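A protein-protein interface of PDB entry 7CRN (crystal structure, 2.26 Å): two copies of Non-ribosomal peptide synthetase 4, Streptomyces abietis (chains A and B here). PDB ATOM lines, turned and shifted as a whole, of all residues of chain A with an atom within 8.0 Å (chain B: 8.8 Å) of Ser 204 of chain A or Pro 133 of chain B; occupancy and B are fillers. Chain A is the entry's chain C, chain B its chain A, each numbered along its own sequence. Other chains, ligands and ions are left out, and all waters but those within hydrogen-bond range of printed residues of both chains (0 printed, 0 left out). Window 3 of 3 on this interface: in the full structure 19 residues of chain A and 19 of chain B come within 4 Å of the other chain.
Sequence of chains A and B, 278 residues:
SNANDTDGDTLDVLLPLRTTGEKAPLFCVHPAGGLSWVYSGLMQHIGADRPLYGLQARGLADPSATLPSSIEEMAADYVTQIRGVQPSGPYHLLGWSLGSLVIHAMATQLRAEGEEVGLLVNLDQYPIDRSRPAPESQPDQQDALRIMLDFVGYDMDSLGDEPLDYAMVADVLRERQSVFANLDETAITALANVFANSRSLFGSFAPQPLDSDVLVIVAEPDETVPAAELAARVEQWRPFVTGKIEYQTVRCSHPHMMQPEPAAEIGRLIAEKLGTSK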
ATOM      1  N   PRO A  68     -40.184 -29.265 -24.268  1.00  0.00           N
ATOM      2  CA  PRO A  68     -38.852 -29.866 -24.119  1.00  0.00           C
ATOM      3  C   PRO A  68     -37.839 -28.810 -23.706  1.00  0.00           C
ATOM      4  O   PRO A  68     -37.929 -27.650 -24.109  1.00  0.00           O
ATOM      5  CB  PRO A  68     -38.554 -30.429 -25.513  1.00  0.00           C
ATOM      6  CG  PRO A  68     -39.448 -29.650 -26.447  1.00  0.00           C
ATOM      7  CD  PRO A  68     -40.679 -29.318 -25.657  1.00  0.00           C
ATOM      8  N   SER A  69     -36.882 -29.211 -22.869  1.00  0.00           N
ATOM      9  CA  SER A  69     -35.850 -28.298 -22.395  1.00  0.00           C
ATOM     10  C   SER A  69     -34.524 -28.483 -23.115  1.00  0.00           C
ATOM     11  O   SER A  69     -33.565 -27.765 -22.813  1.00  0.00           O
ATOM     12  CB  SER A  69     -35.641 -28.453 -20.884  1.00  0.00           C
ATOM     13  OG  SER A  69     -35.524 -29.811 -20.507  1.00  0.00           O
ATOM     14  N   SER A  70     -34.451 -29.406 -24.069  1.00  0.00           N
ATOM     15  CA  SER A  70     -33.243 -29.590 -24.856  1.00  0.00           C
ATOM     16  C   SER A  70     -33.627 -30.086 -26.239  1.00  0.00           C
ATOM     17  O   SER A  70     -34.696 -30.671 -26.442  1.00  0.00           O
ATOM     18  CB  SER A  70     -32.282 -30.575 -24.181  1.00  0.00           C
ATOM     19  OG  SER A  70     -32.824 -31.883 -24.202  1.00  0.00           O
ATOM     20  N   ILE A  71     -32.738 -29.840 -27.202  1.00  0.00           N
ATOM     21  CA  ILE A  71     -32.954 -30.370 -28.543  1.00  0.00           C
ATOM     22  C   ILE A  71     -32.914 -31.894 -28.533  1.00  0.00           C
ATOM     23  O   ILE A  71     -33.620 -32.542 -29.311  1.00  0.00           O
ATOM     24  CB  ILE A  71     -31.929 -29.756 -29.517  1.00  0.00           C
ATOM     25  CG1 ILE A  71     -32.437 -28.390 -29.995  1.00  0.00           C
ATOM     26  CG2 ILE A  71     -31.662 -30.689 -30.699  1.00  0.00           C
ATOM     27  CD1 ILE A  71     -31.382 -27.512 -30.594  1.00  0.00           C
ATOM     28  N   GLU A  72     -32.120 -32.493 -27.638  1.00  0.00           N
ATOM     29  CA  GLU A  72     -32.069 -33.954 -27.554  1.00  0.00           C
ATOM     30  C   GLU A  72     -33.419 -34.534 -27.145  1.00  0.00           C
ATOM     31  O   GLU A  72     -33.860 -35.554 -27.688  1.00  0.00           O
ATOM     32  CB  GLU A  72     -30.981 -34.388 -26.569  1.00  0.00           C
ATOM     33  CG  GLU A  72     -29.549 -34.165 -27.060  1.00  0.00           C
ATOM     34  CD  GLU A  72     -28.979 -32.806 -26.655  1.00  0.00           C
ATOM     35  OE1 GLU A  72     -29.766 -31.902 -26.282  1.00  0.00           O
ATOM     36  OE2 GLU A  72     -27.738 -32.645 -26.710  1.00  0.00           O
ATOM     37  N   LEU A 101     -31.134 -28.502 -36.437  1.00  0.00           N
ATOM     38  CA  LEU A 101     -30.492 -29.027 -35.239  1.00  0.00           C
ATOM     39  C   LEU A 101     -31.217 -30.276 -34.761  1.00  0.00           C
ATOM     40  O   LEU A 101     -30.586 -31.315 -34.512  1.00  0.00           O
ATOM     41  CB  LEU A 101     -30.445 -27.956 -34.145  1.00  0.00           C
ATOM     42  CG  LEU A 101     -29.679 -26.675 -34.493  1.00  0.00           C
ATOM     43  CD1 LEU A 101     -29.572 -25.751 -33.282  1.00  0.00           C
ATOM     44  CD2 LEU A 101     -28.298 -27.002 -35.036  1.00  0.00           C
ATOM     45  N   ILE A 128     -23.791 -23.666 -33.882  1.00  0.00           N
ATOM     46  CA  ILE A 128     -23.822 -22.539 -32.957  1.00  0.00           C
ATOM     47  C   ILE A 128     -22.541 -22.533 -32.135  1.00  0.00           C
ATOM     48  O   ILE A 128     -22.119 -23.575 -31.619  1.00  0.00           O
ATOM     49  CB  ILE A 128     -25.048 -22.625 -32.030  1.00  0.00           C
ATOM     50  CG1 ILE A 128     -26.337 -22.726 -32.850  1.00  0.00           C
ATOM     51  CG2 ILE A 128     -25.082 -21.443 -31.072  1.00  0.00           C
ATOM     52  CD1 ILE A 128     -26.627 -21.491 -33.678  1.00  0.00           C
ATOM     53  N   ASP A 129     -21.928 -21.360 -32.001  1.00  0.00           N
ATOM     54  CA  ASP A 129     -20.863 -21.145 -31.023  1.00  0.00           C
ATOM     55  C   ASP A 129     -21.520 -21.004 -29.652  1.00  0.00           C
ATOM     56  O   ASP A 129     -22.080 -19.955 -29.323  1.00  0.00           O
ATOM     57  CB  ASP A 129     -20.043 -19.912 -31.385  1.00  0.00           C
ATOM     58  CG  ASP A 129     -18.871 -19.681 -30.441  1.00  0.00           C
ATOM     59  OD1 ASP A 129     -18.569 -20.570 -29.614  1.00  0.00           O
ATOM     60  OD2 ASP A 129     -18.251 -18.597 -30.529  1.00  0.00           O
ATOM     61  N   ARG A 130     -21.457 -22.070 -28.848  1.00  0.00           N
ATOM     62  CA  ARG A 130     -22.169 -22.086 -27.573  1.00  0.00           C
ATOM     63  C   ARG A 130     -21.616 -21.066 -26.581  1.00  0.00           C
ATOM     64  O   ARG A 130     -22.336 -20.639 -25.671  1.00  0.00           O
ATOM     65  CB  ARG A 130     -22.107 -23.485 -26.961  1.00  0.00           C
ATOM     66  CG  ARG A 130     -22.824 -24.557 -27.759  1.00  0.00           C
ATOM     67  CD  ARG A 130     -22.886 -25.871 -26.982  1.00  0.00           C
ATOM     68  NE  ARG A 130     -21.565 -26.481 -26.819  1.00  0.00           N
ATOM     69  CZ  ARG A 130     -20.859 -27.040 -27.800  1.00  0.00           C
ATOM     70  NH1 ARG A 130     -19.666 -27.561 -27.538  1.00  0.00           N
ATOM     71  NH2 ARG A 130     -21.338 -27.085 -29.040  1.00  0.00           N
ATOM     72  N   PRO A 133     -23.166 -16.998 -28.835  1.00  0.00           N
ATOM     73  CA  PRO A 133     -24.082 -17.290 -29.948  1.00  0.00           C
ATOM     74  C   PRO A 133     -24.328 -16.098 -30.858  1.00  0.00           C
ATOM     75  O   PRO A 133     -24.842 -15.065 -30.417  1.00  0.00           O
ATOM     76  CB  PRO A 133     -25.367 -17.733 -29.234  1.00  0.00           C
ATOM     77  CG  PRO A 133     -24.915 -18.147 -27.855  1.00  0.00           C
ATOM     78  CD  PRO A 133     -23.822 -17.177 -27.530  1.00  0.00           C
ATOM     79  N   ARG A 199     -35.941 -20.765 -29.063  1.00  0.00           N
ATOM     80  CA  ARG A 199     -34.784 -19.882 -29.016  1.00  0.00           C
ATOM     81  C   ARG A 199     -33.896 -20.192 -27.821  1.00  0.00           C
ATOM     82  O   ARG A 199     -32.669 -20.092 -27.921  1.00  0.00           O
ATOM     83  CB  ARG A 199     -35.238 -18.425 -28.971  1.00  0.00           C
ATOM     84  CG  ARG A 199     -35.402 -17.800 -30.337  1.00  0.00           C
ATOM     85  CD  ARG A 199     -35.028 -16.339 -30.298  1.00  0.00           C
ATOM     86  NE  ARG A 199     -33.583 -16.175 -30.217  1.00  0.00           N
ATOM     87  CZ  ARG A 199     -32.961 -15.006 -30.313  1.00  0.00           C
ATOM     88  NH1 ARG A 199     -31.638 -14.954 -30.226  1.00  0.00           N
ATOM     89  NH2 ARG A 199     -33.662 -13.893 -30.497  1.00  0.00           N
ATOM     90  N   SER A 200     -34.486 -20.595 -26.699  1.00  0.00           N
ATOM     91  CA  SER A 200     -33.640 -20.933 -25.560  1.00  0.00           C
ATOM     92  C   SER A 200     -32.920 -22.261 -25.739  1.00  0.00           C
ATOM     93  O   SER A 200     -32.035 -22.572 -24.937  1.00  0.00           O
ATOM     94  CB  SER A 200     -34.461 -20.972 -24.272  1.00  0.00           C
ATOM     95  OG  SER A 200     -35.137 -22.211 -24.138  1.00  0.00           O
ATOM     96  N   LEU A 201     -33.271 -23.046 -26.757  1.00  0.00           N
ATOM     97  CA  LEU A 201     -32.580 -24.324 -26.945  1.00  0.00           C
ATOM     98  C   LEU A 201     -31.333 -24.265 -27.827  1.00  0.00           C
ATOM     99  O   LEU A 201     -30.553 -25.224 -27.820  1.00  0.00           O
ATOM    100  CB  LEU A 201     -33.509 -25.370 -27.565  1.00  0.00           C
ATOM    101  CG  LEU A 201     -34.855 -25.591 -26.903  1.00  0.00           C
ATOM    102  CD1 LEU A 201     -35.774 -26.358 -27.840  1.00  0.00           C
ATOM    103  CD2 LEU A 201     -34.640 -26.325 -25.608  1.00  0.00           C
ATOM    104  N   PHE A 202     -31.117 -23.184 -28.580  1.00  0.00           N
ATOM    105  CA  PHE A 202     -29.957 -23.123 -29.472  1.00  0.00           C
ATOM    106  C   PHE A 202     -28.632 -23.088 -28.717  1.00  0.00           C
ATOM    107  O   PHE A 202     -27.672 -23.760 -29.111  1.00  0.00           O
ATOM    108  CB  PHE A 202     -30.061 -21.906 -30.389  1.00  0.00           C
ATOM    109  CG  PHE A 202     -30.862 -22.152 -31.629  1.00  0.00           C
ATOM    110  CD1 PHE A 202     -32.236 -22.296 -31.562  1.00  0.00           C
ATOM    111  CD2 PHE A 202     -30.242 -22.237 -32.864  1.00  0.00           C
ATOM    112  CE1 PHE A 202     -32.976 -22.525 -32.705  1.00  0.00           C
ATOM    113  CE2 PHE A 202     -30.975 -22.462 -34.011  1.00  0.00           C
ATOM    114  CZ  PHE A 202     -32.344 -22.606 -33.932  1.00  0.00           C
ATOM    115  N   GLY A 203     -28.546 -22.290 -27.649  1.00  0.00           N
ATOM    116  CA  GLY A 203     -27.279 -22.114 -26.954  1.00  0.00           C
ATOM    117  C   GLY A 203     -26.773 -23.342 -26.221  1.00  0.00           C
ATOM    118  O   GLY A 203     -25.576 -23.425 -25.929  1.00  0.00           O
ATOM    119  N   SER A 204     -27.662 -24.281 -25.913  1.00  0.00           N
ATOM    120  CA  SER A 204     -27.269 -25.466 -25.153  1.00  0.00           C
ATOM    121  C   SER A 204     -27.192 -26.789 -25.915  1.00  0.00           C
ATOM    122  O   SER A 204     -27.056 -27.843 -25.294  1.00  0.00           O
ATOM    123  CB  SER A 204     -28.184 -25.631 -23.933  1.00  0.00           C
ATOM    124  OG  SER A 204     -29.366 -26.333 -24.272  1.00  0.00           O
ATOM    125  N   PHE A 205     -27.274 -26.757 -27.241  1.00  0.00           N
ATOM    126  CA  PHE A 205     -27.187 -28.008 -27.988  1.00  0.00           C
ATOM    127  C   PHE A 205     -25.764 -28.253 -28.475  1.00  0.00           C
ATOM    128  O   PHE A 205     -25.184 -27.417 -29.176  1.00  0.00           O
ATOM    129  CB  PHE A 205     -28.149 -28.000 -29.173  1.00  0.00           C
ATOM    130  CG  PHE A 205     -28.072 -29.244 -30.021  1.00  0.00           C
ATOM    131  CD1 PHE A 205     -28.174 -30.499 -29.441  1.00  0.00           C
ATOM    132  CD2 PHE A 205     -27.895 -29.157 -31.392  1.00  0.00           C
ATOM    133  CE1 PHE A 205     -28.106 -31.643 -30.214  1.00  0.00           C
ATOM    134  CE2 PHE A 205     -27.831 -30.300 -32.171  1.00  0.00           C
ATOM    135  CZ  PHE A 205     -27.940 -31.543 -31.583  1.00  0.00           C
ATOM    136  N   ALA A 206     -25.212 -29.412 -28.110  1.00  0.00           N
ATOM    137  CA  ALA A 206     -23.902 -29.861 -28.575  1.00  0.00           C
ATOM    138  C   ALA A 206     -24.105 -31.037 -29.519  1.00  0.00           C
ATOM    139  O   ALA A 206     -24.356 -32.163 -29.060  1.00  0.00           O
ATOM    140  CB  ALA A 206     -23.010 -30.267 -27.396  1.00  0.00           C
ATOM    141  N   PRO A 207     -24.024 -30.835 -30.830  1.00  0.00           N
ATOM    142  CA  PRO A 207     -24.281 -31.938 -31.757  1.00  0.00           C
ATOM    143  C   PRO A 207     -23.170 -32.975 -31.697  1.00  0.00           C
ATOM    144  O   PRO A 207     -22.005 -32.664 -31.443  1.00  0.00           O
ATOM    145  CB  PRO A 207     -24.337 -31.258 -33.130  1.00  0.00           C
ATOM    146  CG  PRO A 207     -24.495 -29.778 -32.862  1.00  0.00           C
ATOM    147  CD  PRO A 207     -24.021 -29.527 -31.479  1.00  0.00           C
ATOM    148  N   PRO B 127     -28.130 -19.051 -10.256  1.00  0.00           N
ATOM    149  CA  PRO B 127     -27.249 -19.284 -11.410  1.00  0.00           C
ATOM    150  C   PRO B 127     -27.744 -20.418 -12.295  1.00  0.00           C
ATOM    151  O   PRO B 127     -28.406 -21.352 -11.839  1.00  0.00           O
ATOM    152  CB  PRO B 127     -25.903 -19.632 -10.763  1.00  0.00           C
ATOM    153  CG  PRO B 127     -25.942 -18.964  -9.442  1.00  0.00           C
ATOM    154  CD  PRO B 127     -27.377 -19.047  -8.989  1.00  0.00           C
ATOM    155  N   ILE B 128     -27.397 -20.324 -13.579  1.00  0.00           N
ATOM    156  CA  ILE B 128     -27.823 -21.279 -14.599  1.00  0.00           C
ATOM    157  C   ILE B 128     -26.715 -22.302 -14.827  1.00  0.00           C
ATOM    158  O   ILE B 128     -25.539 -21.939 -14.947  1.00  0.00           O
ATOM    159  CB  ILE B 128     -28.162 -20.559 -15.917  1.00  0.00           C
ATOM    160  CG1 ILE B 128     -29.195 -19.453 -15.688  1.00  0.00           C
ATOM    161  CG2 ILE B 128     -28.666 -21.553 -16.948  1.00  0.00           C
ATOM    162  CD1 ILE B 128     -30.456 -19.930 -14.987  1.00  0.00           C
ATOM    163  N   ASP B 129     -27.086 -23.581 -14.887  1.00  0.00           N
ATOM    164  CA  ASP B 129     -26.184 -24.618 -15.390  1.00  0.00           C
ATOM    165  C   ASP B 129     -26.169 -24.515 -16.912  1.00  0.00           C
ATOM    166  O   ASP B 129     -27.082 -24.988 -17.590  1.00  0.00           O
ATOM    167  CB  ASP B 129     -26.636 -25.999 -14.929  1.00  0.00           C
ATOM    168  CG  ASP B 129     -25.666 -27.108 -15.333  1.00  0.00           C
ATOM    169  OD1 ASP B 129     -24.574 -26.808 -15.869  1.00  0.00           O
ATOM    170  OD2 ASP B 129     -26.006 -28.289 -15.113  1.00  0.00           O
ATOM    171  N   ARG B 130     -25.124 -23.895 -17.458  1.00  0.00           N
ATOM    172  CA  ARG B 130     -25.079 -23.633 -18.891  1.00  0.00           C
ATOM    173  C   ARG B 130     -24.983 -24.907 -19.725  1.00  0.00           C
ATOM    174  O   ARG B 130     -25.338 -24.882 -20.910  1.00  0.00           O
ATOM    175  CB  ARG B 130     -23.924 -22.690 -19.210  1.00  0.00           C
ATOM    176  CG  ARG B 130     -24.011 -21.373 -18.456  1.00  0.00           C
ATOM    177  CD  ARG B 130     -23.226 -20.264 -19.149  1.00  0.00           C
ATOM    178  NE  ARG B 130     -21.874 -20.672 -19.525  1.00  0.00           N
ATOM    179  CZ  ARG B 130     -20.924 -21.048 -18.671  1.00  0.00           C
ATOM    180  NH1 ARG B 130     -21.152 -21.072 -17.364  1.00  0.00           N
ATOM    181  NH2 ARG B 130     -19.731 -21.397 -19.130  1.00  0.00           N
ATOM    182  N   SER B 131     -24.505 -26.013 -19.148  1.00  0.00           N
ATOM    183  CA  SER B 131     -24.445 -27.254 -19.909  1.00  0.00           C
ATOM    184  C   SER B 131     -25.797 -27.964 -19.994  1.00  0.00           C
ATOM    185  O   SER B 131     -25.978 -28.803 -20.880  1.00  0.00           O
ATOM    186  CB  SER B 131     -23.388 -28.185 -19.304  1.00  0.00           C
ATOM    187  OG  SER B 131     -23.839 -28.774 -18.097  1.00  0.00           O
ATOM    188  N   ARG B 132     -26.761 -27.627 -19.119  1.00  0.00           N
ATOM    189  CA  ARG B 132     -28.099 -28.221 -19.041  1.00  0.00           C
ATOM    190  C   ARG B 132     -29.025 -27.253 -18.316  1.00  0.00           C
ATOM    191  O   ARG B 132     -29.326 -27.455 -17.133  1.00  0.00           O
ATOM    192  CB  ARG B 132     -28.140 -29.568 -18.302  1.00  0.00           C
ATOM    193  CG  ARG B 132     -26.877 -30.392 -18.318  1.00  0.00           C
ATOM    194  CD  ARG B 132     -27.057 -31.814 -17.805  1.00  0.00           C
ATOM    195  NE  ARG B 132     -25.763 -32.488 -17.849  1.00  0.00           N
ATOM    196  CZ  ARG B 132     -24.756 -32.224 -17.018  1.00  0.00           C
ATOM    197  NH1 ARG B 132     -24.911 -31.323 -16.050  1.00  0.00           N
ATOM    198  NH2 ARG B 132     -23.600 -32.867 -17.135  1.00  0.00           N
ATOM    199  N   PRO B 133     -29.509 -26.204 -18.984  1.00  0.00           N
ATOM    200  CA  PRO B 133     -30.281 -25.177 -18.270  1.00  0.00           C
ATOM    201  C   PRO B 133     -31.613 -25.715 -17.755  1.00  0.00           C
ATOM    202  O   PRO B 133     -32.460 -26.135 -18.546  1.00  0.00           O
ATOM    203  CB  PRO B 133     -30.471 -24.084 -19.333  1.00  0.00           C
ATOM    204  CG  PRO B 133     -29.391 -24.348 -20.350  1.00  0.00           C
ATOM    205  CD  PRO B 133     -29.286 -25.838 -20.393  1.00  0.00           C
ATOM    206  N   ALA B 134     -31.783 -25.743 -16.430  1.00  0.00           N
ATOM    207  CA  ALA B 134     -33.036 -26.171 -15.809  1.00  0.00           C
ATOM    208  C   ALA B 134     -34.180 -25.258 -16.247  1.00  0.00           C
ATOM    209  O   ALA B 134     -34.024 -24.030 -16.221  1.00  0.00           O
ATOM    210  CB  ALA B 134     -32.888 -26.145 -14.288  1.00  0.00           C
ATOM    211  N   PRO B 135     -35.326 -25.803 -16.677  1.00  0.00           N
ATOM    212  CA  PRO B 135     -36.458 -24.921 -17.035  1.00  0.00           C
ATOM    213  C   PRO B 135     -36.956 -24.002 -15.924  1.00  0.00           C
ATOM    214  O   PRO B 135     -37.222 -22.833 -16.200  1.00  0.00           O
ATOM    215  CB  PRO B 135     -37.549 -25.913 -17.504  1.00  0.00           C
ATOM    216  CG  PRO B 135     -37.038 -27.295 -17.152  1.00  0.00           C
ATOM    217  CD  PRO B 135     -35.551 -27.198 -17.094  1.00  0.00           C
ATOM    218  N   GLU B 136     -37.025 -24.523 -14.693  1.00  0.00           N
ATOM    219  CA  GLU B 136     -37.488 -23.769 -13.541  1.00  0.00           C
ATOM    220  C   GLU B 136     -36.598 -22.586 -13.166  1.00  0.00           C
ATOM    221  O   GLU B 136     -37.053 -21.684 -12.462  1.00  0.00           O
ATOM    222  CB  GLU B 136     -37.653 -24.697 -12.333  1.00  0.00           C
ATOM    223  CG  GLU B 136     -36.587 -25.775 -12.229  1.00  0.00           C
ATOM    224  CD  GLU B 136     -36.912 -26.998 -13.064  1.00  0.00           C
ATOM    225  OE1 GLU B 136     -37.926 -27.665 -12.773  1.00  0.00           O
ATOM    226  OE2 GLU B 136     -36.152 -27.291 -14.012  1.00  0.00           O
ATOM    227  N   SER B 137     -35.335 -22.567 -13.628  1.00  0.00           N
ATOM    228  CA  SER B 137     -34.513 -21.457 -13.253  1.00  0.00           C
ATOM    229  C   SER B 137     -34.536 -20.442 -14.365  1.00  0.00           C
ATOM    230  O   SER B 137     -33.826 -19.492 -14.351  1.00  0.00           O
ATOM    231  CB  SER B 137     -33.094 -21.907 -13.071  1.00  0.00           C
ATOM    232  OG  SER B 137     -33.009 -22.931 -12.132  1.00  0.00           O
ATOM    233  N   GLN B 138     -35.373 -20.682 -15.334  1.00  0.00           N
ATOM    234  CA  GLN B 138     -35.473 -19.859 -16.534  1.00  0.00           C
ATOM    235  C   GLN B 138     -36.838 -19.192 -16.590  1.00  0.00           C
ATOM    236  O   GLN B 138     -37.780 -19.642 -15.931  1.00  0.00           O
ATOM    237  CB  GLN B 138     -35.275 -20.720 -17.790  1.00  0.00           C
ATOM    238  CG  GLN B 138     -33.832 -20.909 -18.207  1.00  0.00           C
ATOM    239  CD  GLN B 138     -33.718 -21.859 -19.371  1.00  0.00           C
ATOM    240  OE1 GLN B 138     -33.645 -21.436 -20.526  1.00  0.00           O
ATOM    241  NE2 GLN B 138     -33.724 -23.158 -19.079  1.00  0.00           N
ATOM    242  N   PRO B 139     -36.991 -18.119 -17.365  1.00  0.00           N
ATOM    243  CA  PRO B 139     -38.296 -17.451 -17.416  1.00  0.00           C
ATOM    244  C   PRO B 139     -39.333 -18.316 -18.107  1.00  0.00           C
ATOM    245  O   PRO B 139     -39.046 -19.023 -19.078  1.00  0.00           O
ATOM    246  CB  PRO B 139     -38.023 -16.169 -18.216  1.00  0.00           C
ATOM    247  CG  PRO B 139     -36.537 -16.096 -18.398  1.00  0.00           C
ATOM    248  CD  PRO B 139     -36.003 -17.475 -18.249  1.00  0.00           C
ATOM    249  N   ARG B 199     -34.906 -14.883 -23.176  1.00  0.00           N
ATOM    250  CA  ARG B 199     -34.786 -16.311 -22.917  1.00  0.00           C
ATOM    251  C   ARG B 199     -33.571 -16.896 -23.616  1.00  0.00           C
ATOM    252  O   ARG B 199     -32.949 -17.828 -23.101  1.00  0.00           O
ATOM    253  CB  ARG B 199     -36.048 -17.030 -23.372  1.00  0.00           C
ATOM    254  CG  ARG B 199     -37.082 -17.155 -22.290  1.00  0.00           C
ATOM    255  CD  ARG B 199     -37.840 -18.438 -22.446  1.00  0.00           C
ATOM    256  NE  ARG B 199     -37.047 -19.561 -21.970  1.00  0.00           N
ATOM    257  CZ  ARG B 199     -37.517 -20.794 -21.847  1.00  0.00           C
ATOM    258  NH1 ARG B 199     -36.728 -21.759 -21.402  1.00  0.00           N
ATOM    259  NH2 ARG B 199     -38.780 -21.054 -22.169  1.00  0.00           N
ATOM    260  N   SER B 200     -33.222 -16.369 -24.788  1.00  0.00           N
ATOM    261  CA  SER B 200     -32.014 -16.866 -25.430  1.00  0.00           C
ATOM    262  C   SER B 200     -30.754 -16.351 -24.751  1.00  0.00           C
ATOM    263  O   SER B 200     -29.667 -16.851 -25.057  1.00  0.00           O
ATOM    264  CB  SER B 200     -31.986 -16.499 -26.915  1.00  0.00           C
ATOM    265  OG  SER B 200     -31.484 -15.186 -27.112  1.00  0.00           O
ATOM    266  N   LEU B 201     -30.864 -15.399 -23.816  1.00  0.00           N
ATOM    267  CA  LEU B 201     -29.650 -14.916 -23.158  1.00  0.00           C
ATOM    268  C   LEU B 201     -29.244 -15.739 -21.939  1.00  0.00           C
ATOM    269  O   LEU B 201     -28.085 -15.654 -21.515  1.00  0.00           O
ATOM    270  CB  LEU B 201     -29.823 -13.465 -22.704  1.00  0.00           C
ATOM    271  CG  LEU B 201     -30.168 -12.455 -23.789  1.00  0.00           C
ATOM    272  CD1 LEU B 201     -30.267 -11.073 -23.185  1.00  0.00           C
ATOM    273  CD2 LEU B 201     -29.120 -12.506 -24.882  1.00  0.00           C
ATOM    274  N   PHE B 202     -30.151 -16.513 -21.354  1.00  0.00           N
ATOM    275  CA  PHE B 202     -29.748 -17.445 -20.313  1.00  0.00           C
ATOM    276  C   PHE B 202     -28.931 -18.565 -20.954  1.00  0.00           C
ATOM    277  O   PHE B 202     -28.982 -18.786 -22.166  1.00  0.00           O
ATOM    278  CB  PHE B 202     -30.963 -18.046 -19.594  1.00  0.00           C
ATOM    279  CG  PHE B 202     -31.749 -17.068 -18.755  1.00  0.00           C
ATOM    280  CD1 PHE B 202     -32.507 -16.068 -19.347  1.00  0.00           C
ATOM    281  CD2 PHE B 202     -31.770 -17.185 -17.372  1.00  0.00           C
ATOM    282  CE1 PHE B 202     -33.245 -15.184 -18.576  1.00  0.00           C
ATOM    283  CE2 PHE B 202     -32.508 -16.304 -16.593  1.00  0.00           C
ATOM    284  CZ  PHE B 202     -33.248 -15.302 -17.196  1.00  0.00           C
ATOM    285  N   GLY B 203     -28.175 -19.289 -20.137  1.00  0.00           N
ATOM    286  CA  GLY B 203     -27.356 -20.370 -20.649  1.00  0.00           C
ATOM    287  C   GLY B 203     -26.103 -19.956 -21.385  1.00  0.00           C
ATOM    288  O   GLY B 203     -25.195 -20.780 -21.535  1.00  0.00           O
ATOM    289  N   SER B 204     -26.036 -18.724 -21.888  1.00  0.00           N
ATOM    290  CA  SER B 204     -24.828 -18.209 -22.513  1.00  0.00           C
ATOM    291  C   SER B 204     -24.039 -17.330 -21.557  1.00  0.00           C
ATOM    292  O   SER B 204     -22.855 -17.077 -21.798  1.00  0.00           O
ATOM    293  CB  SER B 204     -25.165 -17.413 -23.784  1.00  0.00           C
ATOM    294  OG  SER B 204     -25.707 -18.262 -24.785  1.00  0.00           O
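OG of Ser 200 of chain A is in hydrogen-bond range of NH1 of Arg 199 of chain B, at 3.2 Å. The side-chain hydroxyl (OG) of Ser 200 of chain B lies within hydrogen-bond range of the guanidinium group (NH1) of Arg 199 of chain A, at 3.1 Å.
O of Pro 133 of chain B lies within hydrogen-bond range of NE2 of Gln 138 of chain B. The backbone carbonyl oxygen of Ala 134 of chain B is in hydrogen-bond range of the side-chain amide nitrogen of Gln 138 of chain B. The side-chain amide oxygen (OE1) of Gln 138 of chain B lies within hydrogen-bond range of the guanidinium group (NH1) of Arg 199 of chain B (3.2 Å).
Pro 135 of chain B touches Ser 69 of chain A. Pro 133 of chain A touches Ser 204 of chain B (CG to OG, 3.2 Å). OE1 of Gln 138 of chain B touches CB of Ser 200 of chain A (3.9 Å). Ser 204 of chain A touches Pro 133 of chain B (CB to CD, 3.7 Å).
Printed residues of chain B within 4 Å of Arg 199 of chain A: Ser 200. Ser 204 of chain A touches one residue of chain B. Arg 130 of chain B touches none of the printed residues of chain A. Pro 133 of chain B touches one residue of chain A. No residue of chain A comes within 4 Å of Ala 134 of chain B. Of the printed residues of chain A, Ser 200 of chain B touches Arg 199 (3.1 Å). The nearest residue of chain B that does not touch Ser 204 of chain A is Arg 130 of chain B (4.2 Å).
Of the 19 printed residues of chain A, 5 touch a printed residue of chain B. Hydrophobic or aromatic side chains of chain A that line the printed part of chain B: Pro 133. Hydrophobic or aromatic side chains of chain B that line the printed part of chain A: Pro 133 and Pro 135. Along chain B the printed residues that touch a printed residue of chain A span positions 133 to 204.
Pro 133 of chain A touches Ser 204 of chain B, and with the chains exchanged Ser 204 of chain A touches Pro 133 of chain B. Arg 199 of chain A touches Ser 200 of chain B, and with the chains exchanged Ser 200 of chain A touches Arg 199 of chain B. Positions printed for both chains: 128, 129, 130, 133, 199, 200, 201, 202, 203 and 204. Of the 6 pairs that touch across the chains among the printed residues, 4 have their exchanged pair printed and touching as well.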
